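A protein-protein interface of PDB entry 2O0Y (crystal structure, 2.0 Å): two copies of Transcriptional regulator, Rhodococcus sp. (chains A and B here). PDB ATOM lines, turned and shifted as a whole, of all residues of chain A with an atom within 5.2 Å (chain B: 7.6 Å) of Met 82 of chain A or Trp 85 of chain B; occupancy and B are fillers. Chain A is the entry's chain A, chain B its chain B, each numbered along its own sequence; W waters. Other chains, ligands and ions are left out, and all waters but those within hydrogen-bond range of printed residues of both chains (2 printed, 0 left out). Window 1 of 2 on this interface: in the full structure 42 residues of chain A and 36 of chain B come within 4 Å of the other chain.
Glu 30 of chain A touches Trp 85 of chain B. Asp 33 of chain A touches Leu 88 of chain B (O to CD1, 3.7 Å). CD1 of Leu 78 of chain A touches CG of Trp 85 of chain B (3.8 Å). Leu 88 of chain B touches Leu 78 of chain A. Ala 89 of chain B touches Leu 83 of chain A. Leu 29 of chain B touches Trp 85 of chain A. Trp 85 of chain A touches Leu 78 of chain B (O to CD1, 3.2 Å). CE of Met 82 of chain B touches CB of Trp 85 of chain A (3.9 Å). Met 82 of chain B touches Val 86 of chain A. N of Val 86 of chain B touches CG1 of Val 86 of chain A (3.6 Å).
Water W1 bridges the backbone carbonyl oxygen (O) of Glu 30 of chain A (2.7 Å) and the guanidinium group (NE) of Arg 84 of chain B (3.2 Å). Water W2 lies within hydrogen-bond range of the side-chain carboxylate of Glu 81 of chain B and the side-chain carboxylate of Glu 30 of chain A.
O of Leu 29 of chain A lies within hydrogen-bond range of NE1 of Trp 85 of chain B (2.9 Å). The side-chain carboxylate of Glu 81 of chain A lies close to the side-chain carboxylate of Glu 30 of chain B (2.9 Å). The side-chain carboxylate (OE2) of Glu 81 of chain B lies close to the side-chain carboxylate (OE2) of Glu 30 of chain A, at 2.5 Å. O of Phe 32 of chain A lies within hydrogen-bond range of NE1 of Trp 85 of chain B, 2.9 Å away. OE2 of Glu 30 of chain A is in salt-bridge range of NH1 of Arg 84 of chain B, 3.3 Å away. The side-chain carboxylate (OE1) of Glu 30 of chain B is in salt-bridge range of the guanidinium group (NH2) of Arg 84 of chain A (3.5 Å).
Of the 17 printed residues of chain A, 12 touch a printed residue of chain B. Hydrophobic or aromatic side chains of chain A that line the printed part of chain B: Ile 26, Leu 29, Leu 78, Met 82, Leu 83, Trp 85 and Val 86. Among the printed residues, Asp or Glu carboxylates within 4 Å of a Lys or Arg side-chain nitrogen of the other chain: Glu 30 of chain A with Arg 84 of chain B and Arg 84 of chain A with Glu 30 of chain B.
Trp 85 of chain B touches six residues of chain A. Of the printed residues of chain B, Phe 32 of chain A touches Trp 85 (2.9 Å). Printed residues of chain B within 4 Å of Arg 84 of chain A: Glu 30. Of the printed residues of chain A, Arg 84 of chain B touches Glu 30 (3.3 Å). The nearest residue of chain B that does not touch Met 82 of chain A is Met 82 of chain B (4.03 Å). The nearest printed residue of chain B that does not touch Arg 84 of chain A is Leu 29 of chain B (4.2 Å).
NE of Arg 84 of chain A lies within salt-bridge range of OE1 of Glu 81 of chain A, at 3.3 Å. N of Glu 81 of chain A sits at hydrogen-bond distance from O of Ser 66 of chain A (2.9 Å). O of Val 67 of chain B lies within hydrogen-bond range of N of Gly 79 of chain B (2.8 Å). OE1 of Glu 81 of chain B lies within salt-bridge range of NH1 of Arg 84 of chain B (3.1 Å). The backbone carbonyl oxygen of Leu 88 of chain B is in hydrogen-bond range of the side-chain hydroxyl of Thr 92 of chain B.
Leu 29 of chain A touches Trp 85 of chain B, and with the chains exchanged Trp 85 of chain A touches Leu 29 of chain B. Glu 30 of chain A touches Trp 85 of chain B, and with the chains exchanged Trp 85 of chain A touches Glu 30 of chain B. Met 82 of chain A touches Trp 85 of chain B, and with the chains exchanged Trp 85 of chain A touches Met 82 of chain B. Val 86 of chain B touches its own counterpart, Val 86 of chain A. 13 positions are printed for both chains.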
ATOM      1  N   ILE A  26     -17.113 -23.204   6.652  1.00  0.00           N
ATOM      2  CA  ILE A  26     -18.011 -22.391   5.814  1.00  0.00           C
ATOM      3  C   ILE A  26     -17.933 -20.914   6.238  1.00  0.00           C
ATOM      4  O   ILE A  26     -17.793 -20.057   5.398  1.00  0.00           O
ATOM      5  CB  ILE A  26     -19.435 -22.903   5.864  1.00  0.00           C
ATOM      6  CG1 ILE A  26     -19.472 -24.309   5.296  1.00  0.00           C
ATOM      7  CG2 ILE A  26     -20.349 -22.035   4.990  1.00  0.00           C
ATOM      8  CD1 ILE A  26     -20.673 -25.073   5.719  1.00  0.00           C
ATOM      9  N   LEU A  29     -14.770 -19.634   4.704  1.00  0.00           N
ATOM     10  CA  LEU A  29     -14.935 -19.401   3.258  1.00  0.00           C
ATOM     11  C   LEU A  29     -15.767 -18.188   2.918  1.00  0.00           C
ATOM     12  O   LEU A  29     -15.540 -17.555   1.866  1.00  0.00           O
ATOM     13  CB  LEU A  29     -15.508 -20.628   2.548  1.00  0.00           C
ATOM     14  CG  LEU A  29     -14.510 -21.789   2.481  1.00  0.00           C
ATOM     15  CD1 LEU A  29     -15.281 -23.139   2.190  1.00  0.00           C
ATOM     16  CD2 LEU A  29     -13.395 -21.468   1.485  1.00  0.00           C
ATOM     17  N   GLU A  30     -16.757 -17.886   3.757  1.00  0.00           N
ATOM     18  CA  GLU A  30     -17.661 -16.774   3.483  1.00  0.00           C
ATOM     19  C   GLU A  30     -16.956 -15.432   3.617  1.00  0.00           C
ATOM     20  O   GLU A  30     -17.477 -14.414   3.181  1.00  0.00           O
ATOM     21  CB  GLU A  30     -18.912 -16.836   4.376  1.00  0.00           C
ATOM     22  CG  GLU A  30     -19.908 -17.934   3.955  1.00  0.00           C
ATOM     23  CD  GLU A  30     -21.082 -17.988   4.879  1.00  0.00           C
ATOM     24  OE1 GLU A  30     -21.072 -17.234   5.863  1.00  0.00           O
ATOM     25  OE2 GLU A  30     -22.008 -18.790   4.663  1.00  0.00           O
ATOM     26  N   PHE A  32     -14.352 -14.738   1.918  1.00  0.00           N
ATOM     27  CA  PHE A  32     -13.827 -14.444   0.616  1.00  0.00           C
ATOM     28  C   PHE A  32     -14.988 -13.998  -0.218  1.00  0.00           C
ATOM     29  O   PHE A  32     -15.980 -14.708  -0.341  1.00  0.00           O
ATOM     30  CB  PHE A  32     -13.194 -15.677  -0.003  1.00  0.00           C
ATOM     31  CG  PHE A  32     -11.978 -16.142   0.705  1.00  0.00           C
ATOM     32  CD1 PHE A  32     -12.058 -17.063   1.738  1.00  0.00           C
ATOM     33  CD2 PHE A  32     -10.728 -15.697   0.294  1.00  0.00           C
ATOM     34  CE1 PHE A  32     -10.895 -17.492   2.412  1.00  0.00           C
ATOM     35  CE2 PHE A  32      -9.573 -16.085   0.927  1.00  0.00           C
ATOM     36  CZ  PHE A  32      -9.638 -17.001   1.998  1.00  0.00           C
ATOM     37  N   ASP A  33     -14.890 -12.800  -0.778  1.00  0.00           N
ATOM     38  CA  ASP A  33     -15.945 -12.308  -1.655  1.00  0.00           C
ATOM     39  C   ASP A  33     -15.289 -11.335  -2.615  1.00  0.00           C
ATOM     40  O   ASP A  33     -14.086 -11.146  -2.524  1.00  0.00           O
ATOM     41  CB  ASP A  33     -17.066 -11.632  -0.844  1.00  0.00           C
ATOM     42  CG  ASP A  33     -16.582 -10.514   0.028  1.00  0.00           C
ATOM     43  OD1 ASP A  33     -15.611  -9.785  -0.317  1.00  0.00           O
ATOM     44  OD2 ASP A  33     -17.219 -10.343   1.094  1.00  0.00           O
ATOM     45  N   SER A  66      -6.421 -28.196  -1.799  1.00  0.00           N
ATOM     46  CA  SER A  66      -6.682 -27.195  -2.873  1.00  0.00           C
ATOM     47  C   SER A  66      -8.017 -26.493  -2.806  1.00  0.00           C
ATOM     48  O   SER A  66      -8.535 -25.974  -3.814  1.00  0.00           O
ATOM     49  CB  SER A  66      -6.450 -27.783  -4.258  1.00  0.00           C
ATOM     50  OG  SER A  66      -5.133 -28.311  -4.299  1.00  0.00           O
ATOM     51  N   VAL A  67      -8.567 -26.403  -1.612  1.00  0.00           N
ATOM     52  CA  VAL A  67      -9.782 -25.628  -1.371  1.00  0.00           C
ATOM     53  C   VAL A  67      -9.430 -24.134  -1.205  1.00  0.00           C
ATOM     54  O   VAL A  67     -10.236 -23.253  -1.532  1.00  0.00           O
ATOM     55  CB  VAL A  67     -10.513 -26.184  -0.118  1.00  0.00           C
ATOM     56  CG1 VAL A  67     -11.571 -25.174   0.412  1.00  0.00           C
ATOM     57  CG2 VAL A  67     -11.105 -27.566  -0.467  1.00  0.00           C
ATOM     58  N   LEU A  78      -9.241 -18.479  -2.776  1.00  0.00           N
ATOM     59  CA  LEU A  78      -9.963 -19.743  -3.042  1.00  0.00           C
ATOM     60  C   LEU A  78      -9.100 -20.596  -3.955  1.00  0.00           C
ATOM     61  O   LEU A  78      -8.506 -20.042  -4.902  1.00  0.00           O
ATOM     62  CB  LEU A  78     -11.307 -19.465  -3.757  1.00  0.00           C
ATOM     63  CG  LEU A  78     -12.386 -18.694  -2.904  1.00  0.00           C
ATOM     64  CD1 LEU A  78     -13.749 -18.750  -3.649  1.00  0.00           C
ATOM     65  CD2 LEU A  78     -12.514 -19.326  -1.511  1.00  0.00           C
ATOM     66  N   GLY A  79      -9.041 -21.901  -3.713  1.00  0.00           N
ATOM     67  CA  GLY A  79      -8.194 -22.760  -4.503  1.00  0.00           C
ATOM     68  C   GLY A  79      -8.939 -23.401  -5.637  1.00  0.00           C
ATOM     69  O   GLY A  79     -10.144 -23.238  -5.765  1.00  0.00           O
ATOM     70  N   PRO A  80      -8.214 -24.117  -6.498  1.00  0.00           N
ATOM     71  CA  PRO A  80      -8.811 -24.652  -7.676  1.00  0.00           C
ATOM     72  C   PRO A  80     -10.003 -25.614  -7.379  1.00  0.00           C
ATOM     73  O   PRO A  80     -10.958 -25.637  -8.164  1.00  0.00           O
ATOM     74  CB  PRO A  80      -7.637 -25.375  -8.388  1.00  0.00           C
ATOM     75  CG  PRO A  80      -6.597 -25.494  -7.438  1.00  0.00           C
ATOM     76  CD  PRO A  80      -6.774 -24.423  -6.406  1.00  0.00           C
ATOM     77  N   GLU A  81      -9.938 -26.409  -6.306  1.00  0.00           N
ATOM     78  CA  GLU A  81     -11.057 -27.337  -6.024  1.00  0.00           C
ATOM     79  C   GLU A  81     -12.310 -26.548  -5.706  1.00  0.00           C
ATOM     80  O   GLU A  81     -13.383 -26.871  -6.200  1.00  0.00           O
ATOM     81  CB  GLU A  81     -10.734 -28.352  -4.906  1.00  0.00           C
ATOM     82  CG  GLU A  81      -9.752 -29.392  -5.387  1.00  0.00           C
ATOM     83  CD  GLU A  81     -10.311 -30.070  -6.648  1.00  0.00           C
ATOM     84  OE1 GLU A  81     -11.406 -30.669  -6.522  1.00  0.00           O
ATOM     85  OE2 GLU A  81      -9.734 -29.880  -7.760  1.00  0.00           O
ATOM     86  N   MET A  82     -12.161 -25.546  -4.865  1.00  0.00           N
ATOM     87  CA  MET A  82     -13.268 -24.658  -4.475  1.00  0.00           C
ATOM     88  C   MET A  82     -13.874 -23.970  -5.707  1.00  0.00           C
ATOM     89  O   MET A  82     -15.060 -23.967  -5.922  1.00  0.00           O
ATOM     90  CB  MET A  82     -12.745 -23.668  -3.438  1.00  0.00           C
ATOM     91  CG  MET A  82     -13.750 -22.718  -2.913  1.00  0.00           C
ATOM     92  SD  MET A  82     -15.191 -23.582  -1.881  1.00  0.00           S
ATOM     93  CE  MET A  82     -16.100 -21.878  -1.708  1.00  0.00           C
ATOM     94  N   LEU A  83     -13.027 -23.439  -6.580  1.00  0.00           N
ATOM     95  CA  LEU A  83     -13.517 -22.809  -7.808  1.00  0.00           C
ATOM     96  C   LEU A  83     -14.238 -23.758  -8.728  1.00  0.00           C
ATOM     97  O   LEU A  83     -15.184 -23.368  -9.438  1.00  0.00           O
ATOM     98  CB  LEU A  83     -12.397 -22.074  -8.534  1.00  0.00           C
ATOM     99  CG  LEU A  83     -11.737 -20.944  -7.723  1.00  0.00           C
ATOM    100  CD1 LEU A  83     -10.399 -20.629  -8.344  1.00  0.00           C
ATOM    101  CD2 LEU A  83     -12.594 -19.682  -7.661  1.00  0.00           C
ATOM    102  N   ARG A  84     -13.804 -25.004  -8.736  1.00  0.00           N
ATOM    103  CA  ARG A  84     -14.485 -26.052  -9.540  1.00  0.00           C
ATOM    104  C   ARG A  84     -15.923 -26.238  -9.028  1.00  0.00           C
ATOM    105  O   ARG A  84     -16.847 -26.398  -9.806  1.00  0.00           O
ATOM    106  CB  ARG A  84     -13.724 -27.369  -9.346  1.00  0.00           C
ATOM    107  CG  ARG A  84     -14.209 -28.464 -10.262  1.00  0.00           C
ATOM    108  CD  ARG A  84     -13.307 -29.756 -10.162  1.00  0.00           C
ATOM    109  NE  ARG A  84     -13.550 -30.587  -8.986  1.00  0.00           N
ATOM    110  CZ  ARG A  84     -14.714 -31.146  -8.643  1.00  0.00           C
ATOM    111  NH1 ARG A  84     -15.812 -30.963  -9.382  1.00  0.00           N
ATOM    112  NH2 ARG A  84     -14.783 -31.922  -7.543  1.00  0.00           N
ATOM    113  N   TRP A  85     -16.092 -26.299  -7.708  1.00  0.00           N
ATOM    114  CA  TRP A  85     -17.442 -26.514  -7.114  1.00  0.00           C
ATOM    115  C   TRP A  85     -18.279 -25.276  -7.408  1.00  0.00           C
ATOM    116  O   TRP A  85     -19.478 -25.384  -7.555  1.00  0.00           O
ATOM    117  CB  TRP A  85     -17.331 -26.656  -5.588  1.00  0.00           C
ATOM    118  CG  TRP A  85     -16.461 -27.875  -5.142  1.00  0.00           C
ATOM    119  CD1 TRP A  85     -16.275 -28.998  -5.804  1.00  0.00           C
ATOM    120  CD2 TRP A  85     -15.727 -27.976  -3.937  1.00  0.00           C
ATOM    121  NE1 TRP A  85     -15.390 -29.835  -5.116  1.00  0.00           N
ATOM    122  CE2 TRP A  85     -15.057 -29.218  -3.953  1.00  0.00           C
ATOM    123  CE3 TRP A  85     -15.573 -27.142  -2.845  1.00  0.00           C
ATOM    124  CZ2 TRP A  85     -14.235 -29.638  -2.927  1.00  0.00           C
ATOM    125  CZ3 TRP A  85     -14.749 -27.558  -1.818  1.00  0.00           C
ATOM    126  CH2 TRP A  85     -14.129 -28.820  -1.855  1.00  0.00           C
ATOM    127  N   VAL A  86     -17.663 -24.090  -7.333  1.00  0.00           N
ATOM    128  CA  VAL A  86     -18.437 -22.826  -7.562  1.00  0.00           C
ATOM    129  C   VAL A  86     -18.961 -22.801  -9.004  1.00  0.00           C
ATOM    130  O   VAL A  86     -20.105 -22.468  -9.279  1.00  0.00           O
ATOM    131  CB  VAL A  86     -17.541 -21.592  -7.285  1.00  0.00           C
ATOM    132  CG1 VAL A  86     -18.220 -20.290  -7.742  1.00  0.00           C
ATOM    133  CG2 VAL A  86     -17.235 -21.542  -5.739  1.00  0.00           C
ATOM    134  N   ARG A  87     -18.112 -23.219  -9.945  1.00  0.00           N
ATOM    135  CA  ARG A  87     -18.488 -23.286 -11.365  1.00  0.00           C
ATOM    136  C   ARG A  87     -19.594 -24.303 -11.586  1.00  0.00           C
ATOM    137  O   ARG A  87     -20.572 -24.056 -12.305  1.00  0.00           O
ATOM    138  CB  ARG A  87     -17.238 -23.733 -12.163  1.00  0.00           C
ATOM    139  CG  ARG A  87     -16.948 -22.996 -13.423  1.00  0.00           C
ATOM    140  CD  ARG A  87     -15.360 -22.917 -13.613  1.00  0.00           C
ATOM    141  NE  ARG A  87     -14.846 -24.285 -13.656  1.00  0.00           N
ATOM    142  CZ  ARG A  87     -13.801 -24.813 -13.001  1.00  0.00           C
ATOM    143  NH1 ARG A  87     -12.942 -24.127 -12.203  1.00  0.00           N
ATOM    144  NH2 ARG A  87     -13.642 -26.090 -13.198  1.00  0.00           N
ATOM    145  N   LEU B  29     -17.913 -33.262  -1.100  1.00  0.00           N
ATOM    146  CA  LEU B  29     -18.023 -32.289  -2.194  1.00  0.00           C
ATOM    147  C   LEU B  29     -17.238 -32.730  -3.411  1.00  0.00           C
ATOM    148  O   LEU B  29     -17.625 -32.496  -4.547  1.00  0.00           O
ATOM    149  CB  LEU B  29     -17.496 -30.950  -1.697  1.00  0.00           C
ATOM    150  CG  LEU B  29     -18.343 -30.219  -0.654  1.00  0.00           C
ATOM    151  CD1 LEU B  29     -17.596 -28.999  -0.090  1.00  0.00           C
ATOM    152  CD2 LEU B  29     -19.636 -29.760  -1.388  1.00  0.00           C
ATOM    153  N   GLU B  30     -16.123 -33.390  -3.183  1.00  0.00           N
ATOM    154  CA  GLU B  30     -15.339 -33.921  -4.326  1.00  0.00           C
ATOM    155  C   GLU B  30     -16.081 -34.913  -5.189  1.00  0.00           C
ATOM    156  O   GLU B  30     -15.688 -35.178  -6.330  1.00  0.00           O
ATOM    157  CB  GLU B  30     -14.071 -34.580  -3.797  1.00  0.00           C
ATOM    158  CG  GLU B  30     -13.115 -33.587  -3.177  1.00  0.00           C
ATOM    159  CD  GLU B  30     -12.257 -32.888  -4.193  1.00  0.00           C
ATOM    160  OE1 GLU B  30     -12.361 -33.215  -5.413  1.00  0.00           O
ATOM    161  OE2 GLU B  30     -11.475 -31.999  -3.783  1.00  0.00           O
ATOM    162  N   VAL B  67     -25.146 -25.515   1.276  1.00  0.00           N
ATOM    163  CA  VAL B  67     -23.954 -26.032   0.547  1.00  0.00           C
ATOM    164  C   VAL B  67     -24.460 -27.134  -0.337  1.00  0.00           C
ATOM    165  O   VAL B  67     -23.921 -27.339  -1.404  1.00  0.00           O
ATOM    166  CB  VAL B  67     -22.841 -26.520   1.580  1.00  0.00           C
ATOM    167  CG1 VAL B  67     -21.853 -27.614   1.032  1.00  0.00           C
ATOM    168  CG2 VAL B  67     -22.081 -25.324   2.196  1.00  0.00           C
ATOM    169  N   LEU B  78     -25.211 -29.412  -5.541  1.00  0.00           N
ATOM    170  CA  LEU B  78     -24.522 -28.350  -4.796  1.00  0.00           C
ATOM    171  C   LEU B  78     -25.612 -27.314  -4.613  1.00  0.00           C
ATOM    172  O   LEU B  78     -26.448 -27.129  -5.515  1.00  0.00           O
ATOM    173  CB  LEU B  78     -23.360 -27.773  -5.632  1.00  0.00           C
ATOM    174  CG  LEU B  78     -22.158 -28.729  -5.855  1.00  0.00           C
ATOM    175  CD1 LEU B  78     -20.989 -27.951  -6.488  1.00  0.00           C
ATOM    176  CD2 LEU B  78     -21.667 -29.263  -4.494  1.00  0.00           C
ATOM    177  N   GLY B  79     -25.602 -26.621  -3.486  1.00  0.00           N
ATOM    178  CA  GLY B  79     -26.744 -25.725  -3.190  1.00  0.00           C
ATOM    179  C   GLY B  79     -26.378 -24.268  -3.362  1.00  0.00           C
ATOM    180  O   GLY B  79     -25.265 -23.928  -3.743  1.00  0.00           O
ATOM    181  N   PRO B  80     -27.351 -23.378  -3.158  1.00  0.00           N
ATOM    182  CA  PRO B  80     -27.201 -21.961  -3.544  1.00  0.00           C
ATOM    183  C   PRO B  80     -26.093 -21.249  -2.820  1.00  0.00           C
ATOM    184  O   PRO B  80     -25.556 -20.256  -3.319  1.00  0.00           O
ATOM    185  CB  PRO B  80     -28.555 -21.347  -3.108  1.00  0.00           C
ATOM    186  CG  PRO B  80     -29.508 -22.508  -3.040  1.00  0.00           C
ATOM    187  CD  PRO B  80     -28.696 -23.717  -2.625  1.00  0.00           C
ATOM    188  N   GLU B  81     -25.686 -21.782  -1.651  1.00  0.00           N
ATOM    189  CA  GLU B  81     -24.531 -21.181  -0.965  1.00  0.00           C
ATOM    190  C   GLU B  81     -23.375 -21.010  -1.882  1.00  0.00           C
ATOM    191  O   GLU B  81     -22.643 -20.024  -1.841  1.00  0.00           O
ATOM    192  CB  GLU B  81     -24.116 -22.042   0.233  1.00  0.00           C
ATOM    193  CG  GLU B  81     -22.773 -21.664   0.930  1.00  0.00           C
ATOM    194  CD  GLU B  81     -22.853 -20.553   1.938  1.00  0.00           C
ATOM    195  OE1 GLU B  81     -23.888 -19.887   1.995  1.00  0.00           O
ATOM    196  OE2 GLU B  81     -21.833 -20.291   2.652  1.00  0.00           O
ATOM    197  N   MET B  82     -23.149 -22.025  -2.716  1.00  0.00           N
ATOM    198  CA  MET B  82     -21.910 -22.024  -3.489  1.00  0.00           C
ATOM    199  C   MET B  82     -21.893 -20.867  -4.495  1.00  0.00           C
ATOM    200  O   MET B  82     -20.859 -20.490  -5.008  1.00  0.00           O
ATOM    201  CB  MET B  82     -21.731 -23.386  -4.230  1.00  0.00           C
ATOM    202  CG  MET B  82     -21.873 -24.632  -3.364  1.00  0.00           C
ATOM    203  SD  MET B  82     -20.474 -24.531  -1.949  1.00  0.00           S
ATOM    204  CE  MET B  82     -19.075 -24.173  -3.158  1.00  0.00           C
ATOM    205  N   LEU B  83     -23.067 -20.360  -4.836  1.00  0.00           N
ATOM    206  CA  LEU B  83     -23.219 -19.276  -5.826  1.00  0.00           C
ATOM    207  C   LEU B  83     -22.672 -17.978  -5.273  1.00  0.00           C
ATOM    208  O   LEU B  83     -22.447 -17.020  -6.013  1.00  0.00           O
ATOM    209  CB  LEU B  83     -24.714 -19.087  -6.167  1.00  0.00           C
ATOM    210  CG  LEU B  83     -25.434 -20.263  -6.837  1.00  0.00           C
ATOM    211  CD1 LEU B  83     -26.906 -19.877  -7.087  1.00  0.00           C
ATOM    212  CD2 LEU B  83     -24.721 -20.601  -8.233  1.00  0.00           C
ATOM    213  N   ARG B  84     -22.464 -17.912  -3.966  1.00  0.00           N
ATOM    214  CA  ARG B  84     -21.999 -16.635  -3.413  1.00  0.00           C
ATOM    215  C   ARG B  84     -20.572 -16.339  -3.769  1.00  0.00           C
ATOM    216  O   ARG B  84     -20.116 -15.199  -3.549  1.00  0.00           O
ATOM    217  CB  ARG B  84     -22.201 -16.571  -1.897  1.00  0.00           C
ATOM    218  CG  ARG B  84     -21.227 -17.398  -1.106  1.00  0.00           C
ATOM    219  CD  ARG B  84     -21.838 -17.632   0.318  1.00  0.00           C
ATOM    220  NE  ARG B  84     -21.720 -16.412   1.118  1.00  0.00           N
ATOM    221  CZ  ARG B  84     -22.495 -16.084   2.155  1.00  0.00           C
ATOM    222  NH1 ARG B  84     -23.494 -16.840   2.526  1.00  0.00           N
ATOM    223  NH2 ARG B  84     -22.273 -14.954   2.795  1.00  0.00           N
ATOM    224  N   TRP B  85     -19.847 -17.329  -4.339  1.00  0.00           N
ATOM    225  CA  TRP B  85     -18.456 -17.070  -4.815  1.00  0.00           C
ATOM    226  C   TRP B  85     -18.333 -16.904  -6.326  1.00  0.00           C
ATOM    227  O   TRP B  85     -17.234 -16.717  -6.848  1.00  0.00           O
ATOM    228  CB  TRP B  85     -17.438 -18.123  -4.259  1.00  0.00           C
ATOM    229  CG  TRP B  85     -17.369 -18.115  -2.742  1.00  0.00           C
ATOM    230  CD1 TRP B  85     -16.747 -17.169  -1.960  1.00  0.00           C
ATOM    231  CD2 TRP B  85     -18.019 -19.023  -1.833  1.00  0.00           C
ATOM    232  NE1 TRP B  85     -16.973 -17.446  -0.612  1.00  0.00           N
ATOM    233  CE2 TRP B  85     -17.741 -18.579  -0.519  1.00  0.00           C
ATOM    234  CE3 TRP B  85     -18.863 -20.130  -2.004  1.00  0.00           C
ATOM    235  CZ2 TRP B  85     -18.219 -19.263   0.613  1.00  0.00           C
ATOM    236  CZ3 TRP B  85     -19.301 -20.834  -0.906  1.00  0.00           C
ATOM    237  CH2 TRP B  85     -18.968 -20.410   0.402  1.00  0.00           C
ATOM    238  N   VAL B  86     -19.465 -16.965  -7.034  1.00  0.00           N
ATOM    239  CA  VAL B  86     -19.502 -16.819  -8.483  1.00  0.00           C
ATOM    240  C   VAL B  86     -18.919 -15.518  -8.953  1.00  0.00           C
ATOM    241  O   VAL B  86     -18.077 -15.528  -9.869  1.00  0.00           O
ATOM    242  CB  VAL B  86     -20.930 -17.012  -9.054  1.00  0.00           C
ATOM    243  CG1 VAL B  86     -21.050 -16.517 -10.517  1.00  0.00           C
ATOM    244  CG2 VAL B  86     -21.299 -18.478  -8.957  1.00  0.00           C
ATOM    245  N   ARG B  87     -19.337 -14.406  -8.349  1.00  0.00           N
ATOM    246  CA  ARG B  87     -18.821 -13.079  -8.796  1.00  0.00           C
ATOM    247  C   ARG B  87     -17.324 -12.961  -8.546  1.00  0.00           C
ATOM    248  O   ARG B  87     -16.578 -12.542  -9.418  1.00  0.00           O
ATOM    249  CB  ARG B  87     -19.541 -11.936  -8.041  1.00  0.00           C
ATOM    250  CG  ARG B  87     -19.148 -10.538  -8.509  1.00  0.00           C
ATOM    251  CD  ARG B  87     -19.664  -9.455  -7.576  1.00  0.00           C
ATOM    252  NE  ARG B  87     -21.120  -9.452  -7.418  1.00  0.00           N
ATOM    253  CZ  ARG B  87     -21.969  -8.615  -8.035  1.00  0.00           C
ATOM    254  NH1 ARG B  87     -21.548  -7.685  -8.870  1.00  0.00           N
ATOM    255  NH2 ARG B  87     -23.267  -8.720  -7.820  1.00  0.00           N
ATOM    256  N   LEU B  88     -16.872 -13.352  -7.360  1.00  0.00           N
ATOM    257  CA  LEU B  88     -15.438 -13.365  -7.050  1.00  0.00           C
ATOM    258  C   LEU B  88     -14.647 -14.254  -8.077  1.00  0.00           C
ATOM    259  O   LEU B  88     -13.620 -13.839  -8.615  1.00  0.00           O
ATOM    260  CB  LEU B  88     -15.237 -13.904  -5.615  1.00  0.00           C
ATOM    261  CG  LEU B  88     -13.819 -14.339  -5.248  1.00  0.00           C
ATOM    262  CD1 LEU B  88     -12.789 -13.136  -5.326  1.00  0.00           C
ATOM    263  CD2 LEU B  88     -13.760 -14.978  -3.901  1.00  0.00           C
ATOM    264  N   ALA B  89     -15.118 -15.484  -8.323  1.00  0.00           N
ATOM    265  CA  ALA B  89     -14.425 -16.383  -9.274  1.00  0.00           C
ATOM    266  C   ALA B  89     -14.255 -15.735 -10.671  1.00  0.00           C
ATOM    267  O   ALA B  89     -13.160 -15.799 -11.311  1.00  0.00           O
ATOM    268  CB  ALA B  89     -15.199 -17.672  -9.401  1.00  0.00           C
ATOM    269  N   GLY B  90     -15.330 -15.117 -11.135  1.00  0.00           N
ATOM    270  CA  GLY B  90     -15.342 -14.459 -12.470  1.00  0.00           C
ATOM    271  C   GLY B  90     -14.352 -13.297 -12.573  1.00  0.00           C
ATOM    272  O   GLY B  90     -13.601 -13.173 -13.551  1.00  0.00           O
ATOM    273  N   ARG B  91     -14.339 -12.457 -11.555  1.00  0.00           N
ATOM    274  CA  ARG B  91     -13.463 -11.291 -11.513  1.00  0.00           C
ATOM    275  C   ARG B  91     -11.989 -11.637 -11.372  1.00  0.00           C
ATOM    276  O   ARG B  91     -11.126 -10.868 -11.764  1.00  0.00           O
ATOM    277  CB  ARG B  91     -13.870 -10.392 -10.355  1.00  0.00           C
ATOM    278  CG  ARG B  91     -15.247  -9.769 -10.539  1.00  0.00           C
ATOM    279  CD  ARG B  91     -15.706  -9.121  -9.252  1.00  0.00           C
ATOM    280  NE  ARG B  91     -14.788  -8.088  -8.770  1.00  0.00           N
ATOM    281  CZ  ARG B  91     -14.972  -6.785  -8.954  1.00  0.00           C
ATOM    282  NH1 ARG B  91     -16.029  -6.366  -9.634  1.00  0.00           N
ATOM    283  NH2 ARG B  91     -14.095  -5.905  -8.473  1.00  0.00           N
ATOM    284  N   THR B  92     -11.681 -12.766 -10.754  1.00  0.00           N
ATOM    285  CA  THR B  92     -10.281 -13.103 -10.526  1.00  0.00           C
ATOM    286  C   THR B  92      -9.800 -14.200 -11.450  1.00  0.00           C
ATOM    287  O   THR B  92      -8.685 -14.578 -11.349  1.00  0.00           O
ATOM    288  CB  THR B  92     -10.007 -13.550  -9.074  1.00  0.00           C
ATOM    289  OG1 THR B  92     -10.814 -14.687  -8.741  1.00  0.00           O
ATOM    290  CG2 THR B  92     -10.291 -12.395  -8.076  1.00  0.00           C
HETATM  291  O   HOH W   1     -19.286 -14.409   1.147  1.00  0.00           O
HETATM  292  O   HOH W   2     -24.937 -20.068   4.793  1.00  0.00           O
